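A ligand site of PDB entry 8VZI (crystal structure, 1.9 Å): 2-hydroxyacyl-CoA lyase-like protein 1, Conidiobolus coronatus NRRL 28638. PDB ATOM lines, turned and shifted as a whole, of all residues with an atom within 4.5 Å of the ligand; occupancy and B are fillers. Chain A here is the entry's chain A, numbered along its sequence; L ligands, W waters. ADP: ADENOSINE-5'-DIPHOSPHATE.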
ATOM      1  N   ASN A  93      14.011  11.977  -3.502  1.00  0.00           N
ATOM      2  CA  ASN A  93      13.083  11.070  -4.176  1.00  0.00           C
ATOM      3  C   ASN A  93      12.806   9.819  -3.353  1.00  0.00           C
ATOM      4  O   ASN A  93      11.887   9.072  -3.715  1.00  0.00           O
ATOM      5  CB  ASN A  93      13.613  10.640  -5.542  1.00  0.00           C
ATOM      6  CG  ASN A  93      13.413  11.685  -6.625  1.00  0.00           C
ATOM      7  OD1 ASN A  93      12.605  12.616  -6.475  1.00  0.00           O
ATOM      8  ND2 ASN A  93      14.099  11.512  -7.755  1.00  0.00           N
ATOM      9  N   CYS A  94      13.574   9.580  -2.280  1.00  0.00           N
ATOM     10  CA  CYS A  94      13.478   8.379  -1.473  1.00  0.00           C
ATOM     11  C   CYS A  94      13.823   7.140  -2.311  1.00  0.00           C
ATOM     12  O   CYS A  94      13.076   6.165  -2.368  1.00  0.00           O
ATOM     13  CB  CYS A  94      12.097   8.259  -0.828  1.00  0.00           C
ATOM     14  SG  CYS A  94      11.700   9.708   0.203  1.00  0.00           S
ATOM     15  N   ARG A 154      12.058   3.948   4.721  1.00  0.00           N
ATOM     16  CA  ARG A 154      12.074   4.887   3.607  1.00  0.00           C
ATOM     17  C   ARG A 154      13.397   4.732   2.875  1.00  0.00           C
ATOM     18  O   ARG A 154      14.457   4.945   3.477  1.00  0.00           O
ATOM     19  CB  ARG A 154      11.897   6.317   4.096  1.00  0.00           C
ATOM     20  CG  ARG A 154      12.174   7.377   3.024  1.00  0.00           C
ATOM     21  CD  ARG A 154      11.979   8.779   3.584  1.00  0.00           C
ATOM     22  NE  ARG A 154      10.569   9.126   3.737  1.00  0.00           N
ATOM     23  CZ  ARG A 154      10.132  10.316   4.144  1.00  0.00           C
ATOM     24  NH1 ARG A 154      10.965  11.266   4.525  1.00  0.00           N
ATOM     25  NH2 ARG A 154       8.833  10.569   4.120  1.00  0.00           N
ATOM     26  N   PRO A 155      13.393   4.332   1.604  1.00  0.00           N
ATOM     27  CA  PRO A 155      14.666   4.146   0.889  1.00  0.00           C
ATOM     28  C   PRO A 155      15.380   5.483   0.714  1.00  0.00           C
ATOM     29  O   PRO A 155      14.763   6.549   0.727  1.00  0.00           O
ATOM     30  CB  PRO A 155      14.237   3.562  -0.466  1.00  0.00           C
ATOM     31  CG  PRO A 155      12.843   3.000  -0.215  1.00  0.00           C
ATOM     32  CD  PRO A 155      12.238   3.978   0.760  1.00  0.00           C
ATOM     33  N   TYR A 185       9.100  -5.861   6.062  1.00  0.00           N
ATOM     34  CA  TYR A 185       8.120  -4.792   6.016  1.00  0.00           C
ATOM     35  C   TYR A 185       7.125  -4.952   7.159  1.00  0.00           C
ATOM     36  O   TYR A 185       7.130  -5.948   7.893  1.00  0.00           O
ATOM     37  CB  TYR A 185       7.408  -4.748   4.664  1.00  0.00           C
ATOM     38  CG  TYR A 185       8.271  -4.093   3.605  1.00  0.00           C
ATOM     39  CD1 TYR A 185       8.703  -2.780   3.776  1.00  0.00           C
ATOM     40  CD2 TYR A 185       8.674  -4.774   2.458  1.00  0.00           C
ATOM     41  CE1 TYR A 185       9.511  -2.157   2.836  1.00  0.00           C
ATOM     42  CE2 TYR A 185       9.478  -4.154   1.510  1.00  0.00           C
ATOM     43  CZ  TYR A 185       9.896  -2.839   1.707  1.00  0.00           C
ATOM     44  OH  TYR A 185      10.694  -2.198   0.776  1.00  0.00           O
ATOM     45  N   GLY A 211       1.192   8.062  -5.230  1.00  0.00           N
ATOM     46  CA  GLY A 211       2.487   8.657  -5.479  1.00  0.00           C
ATOM     47  C   GLY A 211       3.536   7.626  -5.862  1.00  0.00           C
ATOM     48  O   GLY A 211       3.282   6.428  -5.969  1.00  0.00           O
ATOM     49  N   LYS A 212       4.765   8.126  -6.066  1.00  0.00           N
ATOM     50  CA  LYS A 212       5.812   7.236  -6.540  1.00  0.00           C
ATOM     51  C   LYS A 212       6.331   6.306  -5.445  1.00  0.00           C
ATOM     52  O   LYS A 212       7.095   5.387  -5.762  1.00  0.00           O
ATOM     53  CB  LYS A 212       6.972   8.037  -7.177  1.00  0.00           C
ATOM     54  CG  LYS A 212       7.767   8.966  -6.272  1.00  0.00           C
ATOM     55  CD  LYS A 212       8.926   9.591  -7.073  1.00  0.00           C
ATOM     56  CE  LYS A 212       9.896  10.393  -6.179  1.00  0.00           C
ATOM     57  NZ  LYS A 212       9.225  11.559  -5.510  1.00  0.00           N
ATOM     58  N   GLY A 213       5.901   6.491  -4.200  1.00  0.00           N
ATOM     59  CA  GLY A 213       6.126   5.451  -3.207  1.00  0.00           C
ATOM     60  C   GLY A 213       5.324   4.212  -3.536  1.00  0.00           C
ATOM     61  O   GLY A 213       5.794   3.076  -3.349  1.00  0.00           O
ATOM     62  N   TYR A 216       7.103   2.525  -6.578  1.00  0.00           N
ATOM     63  CA  TYR A 216       8.322   1.896  -6.086  1.00  0.00           C
ATOM     64  C   TYR A 216       8.012   0.574  -5.383  1.00  0.00           C
ATOM     65  O   TYR A 216       8.683  -0.436  -5.601  1.00  0.00           O
ATOM     66  CB  TYR A 216       9.094   2.832  -5.141  1.00  0.00           C
ATOM     67  CG  TYR A 216      10.293   2.136  -4.542  1.00  0.00           C
ATOM     68  CD1 TYR A 216      11.426   1.921  -5.308  1.00  0.00           C
ATOM     69  CD2 TYR A 216      10.257   1.604  -3.244  1.00  0.00           C
ATOM     70  CE1 TYR A 216      12.518   1.248  -4.799  1.00  0.00           C
ATOM     71  CE2 TYR A 216      11.348   0.931  -2.736  1.00  0.00           C
ATOM     72  CZ  TYR A 216      12.482   0.756  -3.515  1.00  0.00           C
ATOM     73  OH  TYR A 216      13.590   0.084  -3.047  1.00  0.00           O
ATOM     74  N   SER A 217       6.983   0.565  -4.524  1.00  0.00           N
ATOM     75  CA  SER A 217       6.632  -0.634  -3.792  1.00  0.00           C
ATOM     76  C   SER A 217       5.904  -1.649  -4.659  1.00  0.00           C
ATOM     77  O   SER A 217       5.621  -2.754  -4.172  1.00  0.00           O
ATOM     78  CB  SER A 217       5.762  -0.288  -2.586  1.00  0.00           C
ATOM     79  OG  SER A 217       4.453   0.054  -2.982  1.00  0.00           O
ATOM     80  N   THR A 237       0.379  11.031  -8.934  1.00  0.00           N
ATOM     81  CA  THR A 237       1.435  12.018  -9.060  1.00  0.00           C
ATOM     82  C   THR A 237       2.224  11.733 -10.335  1.00  0.00           C
ATOM     83  O   THR A 237       2.072  10.665 -10.948  1.00  0.00           O
ATOM     84  CB  THR A 237       2.339  12.005  -7.823  1.00  0.00           C
ATOM     85  OG1 THR A 237       3.117  10.800  -7.814  1.00  0.00           O
ATOM     86  CG2 THR A 237       1.504  12.118  -6.551  1.00  0.00           C
ATOM     87  N   GLY A 270       1.753   6.477  -0.694  1.00  0.00           N
ATOM     88  CA  GLY A 270       3.111   6.781  -1.091  1.00  0.00           C
ATOM     89  C   GLY A 270       3.275   8.149  -1.711  1.00  0.00           C
ATOM     90  O   GLY A 270       3.898   8.294  -2.769  1.00  0.00           O
ATOM     91  N   ALA A 271       2.728   9.171  -1.062  1.00  0.00           N
ATOM     92  CA  ALA A 271       2.799  10.529  -1.567  1.00  0.00           C
ATOM     93  C   ALA A 271       2.818  11.467  -0.382  1.00  0.00           C
ATOM     94  O   ALA A 271       2.111  11.249   0.608  1.00  0.00           O
ATOM     95  CB  ALA A 271       1.610  10.844  -2.489  1.00  0.00           C
ATOM     96  N   ARG A 272       3.641  12.506  -0.462  1.00  0.00           N
ATOM     97  CA  ARG A 272       3.770  13.433   0.652  1.00  0.00           C
ATOM     98  C   ARG A 272       2.984  14.703   0.379  1.00  0.00           C
ATOM     99  O   ARG A 272       2.817  15.129  -0.764  1.00  0.00           O
ATOM    100  CB  ARG A 272       5.234  13.789   0.914  1.00  0.00           C
ATOM    101  CG  ARG A 272       6.022  12.631   1.450  1.00  0.00           C
ATOM    102  CD  ARG A 272       7.472  13.025   1.581  1.00  0.00           C
ATOM    103  NE  ARG A 272       8.138  12.950   0.280  1.00  0.00           N
ATOM    104  CZ  ARG A 272       9.451  12.983   0.114  1.00  0.00           C
ATOM    105  NH1 ARG A 272      10.274  13.159   1.138  1.00  0.00           N
ATOM    106  NH2 ARG A 272       9.944  12.827  -1.108  1.00  0.00           N
ATOM    107  N   ASN A 274       3.984  17.563   0.582  1.00  0.00           N
ATOM    108  CA  ASN A 274       5.030  18.568   0.487  1.00  0.00           C
ATOM    109  C   ASN A 274       4.646  19.588  -0.575  1.00  0.00           C
ATOM    110  O   ASN A 274       3.450  19.779  -0.839  1.00  0.00           O
ATOM    111  CB  ASN A 274       6.396  17.917   0.185  1.00  0.00           C
ATOM    112  CG  ASN A 274       6.423  17.172  -1.149  1.00  0.00           C
ATOM    113  OD1 ASN A 274       5.446  17.159  -1.882  1.00  0.00           O
ATOM    114  ND2 ASN A 274       7.563  16.550  -1.468  1.00  0.00           N
ATOM    115  N   MET A 276       4.584  19.573  -3.684  1.00  0.00           N
ATOM    116  CA  MET A 276       3.850  19.074  -4.856  1.00  0.00           C
ATOM    117  C   MET A 276       2.352  19.043  -4.612  1.00  0.00           C
ATOM    118  O   MET A 276       1.570  19.167  -5.562  1.00  0.00           O
ATOM    119  CB  MET A 276       4.356  17.693  -5.247  1.00  0.00           C
ATOM    120  CG  MET A 276       5.687  17.742  -5.950  1.00  0.00           C
ATOM    121  SD  MET A 276       6.430  16.156  -6.336  1.00  0.00           S
ATOM    122  CE  MET A 276       5.029  15.264  -7.065  1.00  0.00           C
ATOM    123  N   VAL A 292      -0.919   6.561   4.106  1.00  0.00           N
ATOM    124  CA  VAL A 292      -0.223   5.273   4.128  1.00  0.00           C
ATOM    125  C   VAL A 292       1.240   5.550   3.813  1.00  0.00           C
ATOM    126  O   VAL A 292       1.589   5.919   2.691  1.00  0.00           O
ATOM    127  CB  VAL A 292      -0.821   4.274   3.119  1.00  0.00           C
ATOM    128  CG1 VAL A 292      -0.205   2.908   3.320  1.00  0.00           C
ATOM    129  CG2 VAL A 292      -2.348   4.202   3.243  1.00  0.00           C
ATOM    130  N   ASP A 293       2.104   5.365   4.810  1.00  0.00           N
ATOM    131  CA  ASP A 293       3.522   5.619   4.598  1.00  0.00           C
ATOM    132  C   ASP A 293       4.330   4.711   5.512  1.00  0.00           C
ATOM    133  O   ASP A 293       3.872   4.313   6.584  1.00  0.00           O
ATOM    134  CB  ASP A 293       3.856   7.100   4.837  1.00  0.00           C
ATOM    135  CG  ASP A 293       5.042   7.564   4.025  1.00  0.00           C
ATOM    136  OD1 ASP A 293       6.163   7.097   4.308  1.00  0.00           O
ATOM    137  OD2 ASP A 293       4.853   8.384   3.093  1.00  0.00           O
ATOM    138  N   ILE A 294       5.554   4.396   5.070  1.00  0.00           N
ATOM    139  CA  ILE A 294       6.492   3.638   5.887  1.00  0.00           C
ATOM    140  C   ILE A 294       7.327   4.522   6.814  1.00  0.00           C
ATOM    141  O   ILE A 294       8.059   3.997   7.661  1.00  0.00           O
ATOM    142  CB  ILE A 294       7.407   2.822   4.945  1.00  0.00           C
ATOM    143  CG1 ILE A 294       8.073   1.669   5.704  1.00  0.00           C
ATOM    144  CG2 ILE A 294       8.410   3.724   4.220  1.00  0.00           C
ATOM    145  CD1 ILE A 294       8.696   0.642   4.783  1.00  0.00           C
ATOM    146  N   SER A 295       7.260   5.848   6.661  1.00  0.00           N
ATOM    147  CA  SER A 295       8.012   6.765   7.507  1.00  0.00           C
ATOM    148  C   SER A 295       7.044   7.391   8.499  1.00  0.00           C
ATOM    149  O   SER A 295       6.272   8.289   8.122  1.00  0.00           O
ATOM    150  CB  SER A 295       8.697   7.852   6.668  1.00  0.00           C
ATOM    151  OG  SER A 295       9.354   8.819   7.499  1.00  0.00           O
ATOM    152  N   GLY A 311       2.663   1.307   7.354  1.00  0.00           N
ATOM    153  CA  GLY A 311       2.720  -0.003   6.747  1.00  0.00           C
ATOM    154  C   GLY A 311       3.100   0.042   5.275  1.00  0.00           C
ATOM    155  O   GLY A 311       3.105   1.102   4.638  1.00  0.00           O
ATOM    156  N   ASN A 312       3.416  -1.136   4.764  1.00  0.00           N
ATOM    157  CA  ASN A 312       3.774  -1.306   3.361  1.00  0.00           C
ATOM    158  C   ASN A 312       2.567  -1.085   2.466  1.00  0.00           C
ATOM    159  O   ASN A 312       1.499  -1.670   2.696  1.00  0.00           O
ATOM    160  CB  ASN A 312       4.345  -2.707   3.155  1.00  0.00           C
ATOM    161  CG  ASN A 312       5.276  -2.788   1.960  1.00  0.00           C
ATOM    162  OD1 ASN A 312       6.043  -1.868   1.706  1.00  0.00           O
ATOM    163  ND2 ASN A 312       5.199  -3.887   1.219  1.00  0.00           N
ATOM    164  N   ILE A 313       2.735  -0.276   1.418  1.00  0.00           N
ATOM    165  CA  ILE A 313       1.603   0.103   0.577  1.00  0.00           C
ATOM    166  C   ILE A 313       0.886  -1.096  -0.042  1.00  0.00           C
ATOM    167  O   ILE A 313      -0.347  -1.153   0.036  1.00  0.00           O
ATOM    168  CB  ILE A 313       2.033   1.138  -0.475  1.00  0.00           C
ATOM    169  CG1 ILE A 313       2.269   2.491   0.190  1.00  0.00           C
ATOM    170  CG2 ILE A 313       0.956   1.296  -1.542  1.00  0.00           C
ATOM    171  CD1 ILE A 313       3.166   3.406  -0.613  1.00  0.00           C
ATOM    172  N   THR A 414      11.110  15.277  -7.013  1.00  0.00           N
ATOM    173  CA  THR A 414      10.860  16.090  -5.822  1.00  0.00           C
ATOM    174  C   THR A 414      11.752  17.335  -5.796  1.00  0.00           C
ATOM    175  O   THR A 414      11.363  18.359  -5.217  1.00  0.00           O
ATOM    176  CB  THR A 414      11.057  15.217  -4.585  1.00  0.00           C
ATOM    177  OG1 THR A 414      10.124  14.122  -4.612  1.00  0.00           O
ATOM    178  CG2 THR A 414      10.855  16.021  -3.285  1.00  0.00           C
HETATM  179  PB  ADP L   1       5.320  11.902  -4.925  1.00  0.00           P
HETATM  180  O1B ADP L   1       6.472  12.821  -5.331  1.00  0.00           O
HETATM  181  O2B ADP L   1       4.886  10.924  -6.012  1.00  0.00           O
HETATM  182  O3B ADP L   1       4.143  12.593  -4.259  1.00  0.00           O
HETATM  183  PA  ADP L   1       6.951  11.389  -2.658  1.00  0.00           P
HETATM  184  O1A ADP L   1       8.360  11.051  -3.048  1.00  0.00           O
HETATM  185  O2A ADP L   1       6.522  12.747  -2.176  1.00  0.00           O
HETATM  186  O3A ADP L   1       5.944  10.906  -3.824  1.00  0.00           O
HETATM  187  O5' ADP L   1       6.516  10.367  -1.486  1.00  0.00           O
HETATM  188  C5' ADP L   1       7.052   9.047  -1.438  1.00  0.00           C
HETATM  189  C4' ADP L   1       6.653   8.482  -0.087  1.00  0.00           C
HETATM  190  O4' ADP L   1       6.495   7.063  -0.178  1.00  0.00           O
HETATM  191  C3' ADP L   1       7.728   8.730   0.966  1.00  0.00           C
HETATM  192  O3' ADP L   1       7.088   9.481   1.997  1.00  0.00           O
HETATM  193  C2' ADP L   1       8.136   7.363   1.478  1.00  0.00           C
HETATM  194  O2' ADP L   1       8.327   7.334   2.903  1.00  0.00           O
HETATM  195  C1' ADP L   1       6.955   6.495   1.051  1.00  0.00           C
HETATM  196  N9  ADP L   1       7.309   5.079   0.806  1.00  0.00           N
HETATM  197  C8  ADP L   1       8.363   4.599   0.136  1.00  0.00           C
HETATM  198  N7  ADP L   1       8.345   3.237   0.109  1.00  0.00           N
HETATM  199  C5  ADP L   1       7.236   2.836   0.761  1.00  0.00           C
HETATM  200  C6  ADP L   1       6.604   1.533   1.106  1.00  0.00           C
HETATM  201  N6  ADP L   1       7.167   0.360   0.736  1.00  0.00           N
HETATM  202  N1  ADP L   1       5.458   1.564   1.815  1.00  0.00           N
HETATM  203  C2  ADP L   1       4.894   2.723   2.212  1.00  0.00           C
HETATM  204  N3  ADP L   1       5.407   3.938   1.929  1.00  0.00           N
HETATM  205  C4  ADP L   1       6.558   4.058   1.223  1.00  0.00           C
HETATM  206  O   HOH W   1       5.907  11.535  -8.733  1.00  0.00           O
HETATM  207  O   HOH W   2       8.011  -2.229  -0.578  1.00  0.00           O
HETATM  208  O   HOH W   3       9.886   0.736   0.096  1.00  0.00           O
HETATM  209  O   HOH W   4       7.637  14.730  -3.752  1.00  0.00           O
HETATM  210  O   HOH W   5       7.764  13.067  -7.616  1.00  0.00           O
HETATM  211  O   HOH W   6       4.135  14.870  -3.034  1.00  0.00           O
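N1 of the ligand sits at hydrogen-bond distance from N of Ile 313 (3.3 Å). NH2 of Arg 154 lies within hydrogen-bond range of O3' of the ligand, 3.0 Å away. OD1 of Asp 293 is in hydrogen-bond range of O2' of the ligand (2.6 Å). N3 of the ligand lies within hydrogen-bond range of N of Ile 294. The side-chain hydroxyl (OG1) of Thr 237 sits at hydrogen-bond distance from an oxygen (O2B) of the ligand. The guanidinium group of Arg 272 lies within salt-bridge range of an oxygen (O2A) of the ligand, 2.9 Å away. The side-chain amino group (NZ) of Lys 212 is in salt-bridge range of an oxygen (O1A) of the ligand (2.7 Å). N6 of the ligand is in hydrogen-bond range of OD1 of Asn 312, 2.7 Å away. The backbone NH of Arg 272 is in hydrogen-bond range of an oxygen (O2A) of the ligand, at 3.4 Å. The backbone NH (N) of Lys 212 lies within hydrogen-bond range of an oxygen (O2B) of the ligand (2.8 Å).
The backbone carbonyl oxygen (O) of Gly 213 is in hydrogen-bond range of the side-chain hydroxyl (OG) of Ser 217. The side-chain amide oxygen (OD1) of Asn 93 is in hydrogen-bond range of the backbone NH (N) of Thr 414, at 3.1 Å. The backbone NH of Gly 213 lies within hydrogen-bond range of the backbone carbonyl oxygen of Gly 270, at 3.1 Å. The backbone NH (N) of Lys 212 lies within hydrogen-bond range of the backbone carbonyl oxygen (O) of Gly 270, at 3.4 Å. NE of Arg 154 lies close to SG of Cys 94 (3.8 Å). OG1 of Thr 414 sits at hydrogen-bond distance from NZ of Lys 212 (2.9 Å). N of Ser 295 is in hydrogen-bond range of OD1 of Asp 293. The backbone NH (N) of Gly 270 is in hydrogen-bond range of the backbone carbonyl oxygen (O) of Val 292 (3.4 Å).
An oxygen (O3A) of the ligand sits close to the backbone carbonyl oxygen (O) of Gly 270, at 3.5 Å. SD of Met 276 sits close to O1B of the ligand, 3.5 Å away. Residues that only touch the ligand: Pro 155 (3.97 Å), Gly 211 (3.3 Å), Gly 213 (3.5 Å), Ser 217 (3.7 Å), Ala 271 (3.6 Å), Ser 295 (3.8 Å), Gly 311 (3.4 Å) and Thr 414 (3.9 Å). 18 residues have an atom within 4 Å of the ligand: Arg 154, Pro 155, Gly 211, Lys 212, Gly 213, Ser 217, Thr 237, Gly 270, Ala 271, Arg 272, Met 276, Asp 293, Ile 294, Ser 295, Gly 311, Asn 312, Ile 313 and Thr 414.
Water W6 lies within hydrogen-bond range of an oxygen (O3B) of the ligand, the backbone carbonyl oxygen (O) of Arg 272 and the side-chain amide oxygen (OD1) of Asn 274. Water W5 lies within hydrogen-bond range of an oxygen (O1B) of the ligand (2.6 Å), the side-chain amino group (NZ) of Lys 212 (3.0 Å) and the side-chain sulfur (SD) of Met 276 (3.6 Å). Water W4 lies within hydrogen-bond range of OG1 of Thr 414 (2.7 Å), O1B of the ligand (2.7 Å), ND2 of Asn 274 (2.9 Å) and SD of Met 276 (3.2 Å). Water W3 bridges a nitrogen (N6) of the ligand (2.8 Å) and the side-chain hydroxyl (OH) of Tyr 185 (3.1 Å). Water W1 lies within hydrogen-bond range of O2B of the ligand and OG1 of Thr 237. Water W2 lies within hydrogen-bond range of OH of Tyr 185 (3.0 Å), N6 of the ligand (3.0 Å) and OD1 of Asn 312 (3.0 Å).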
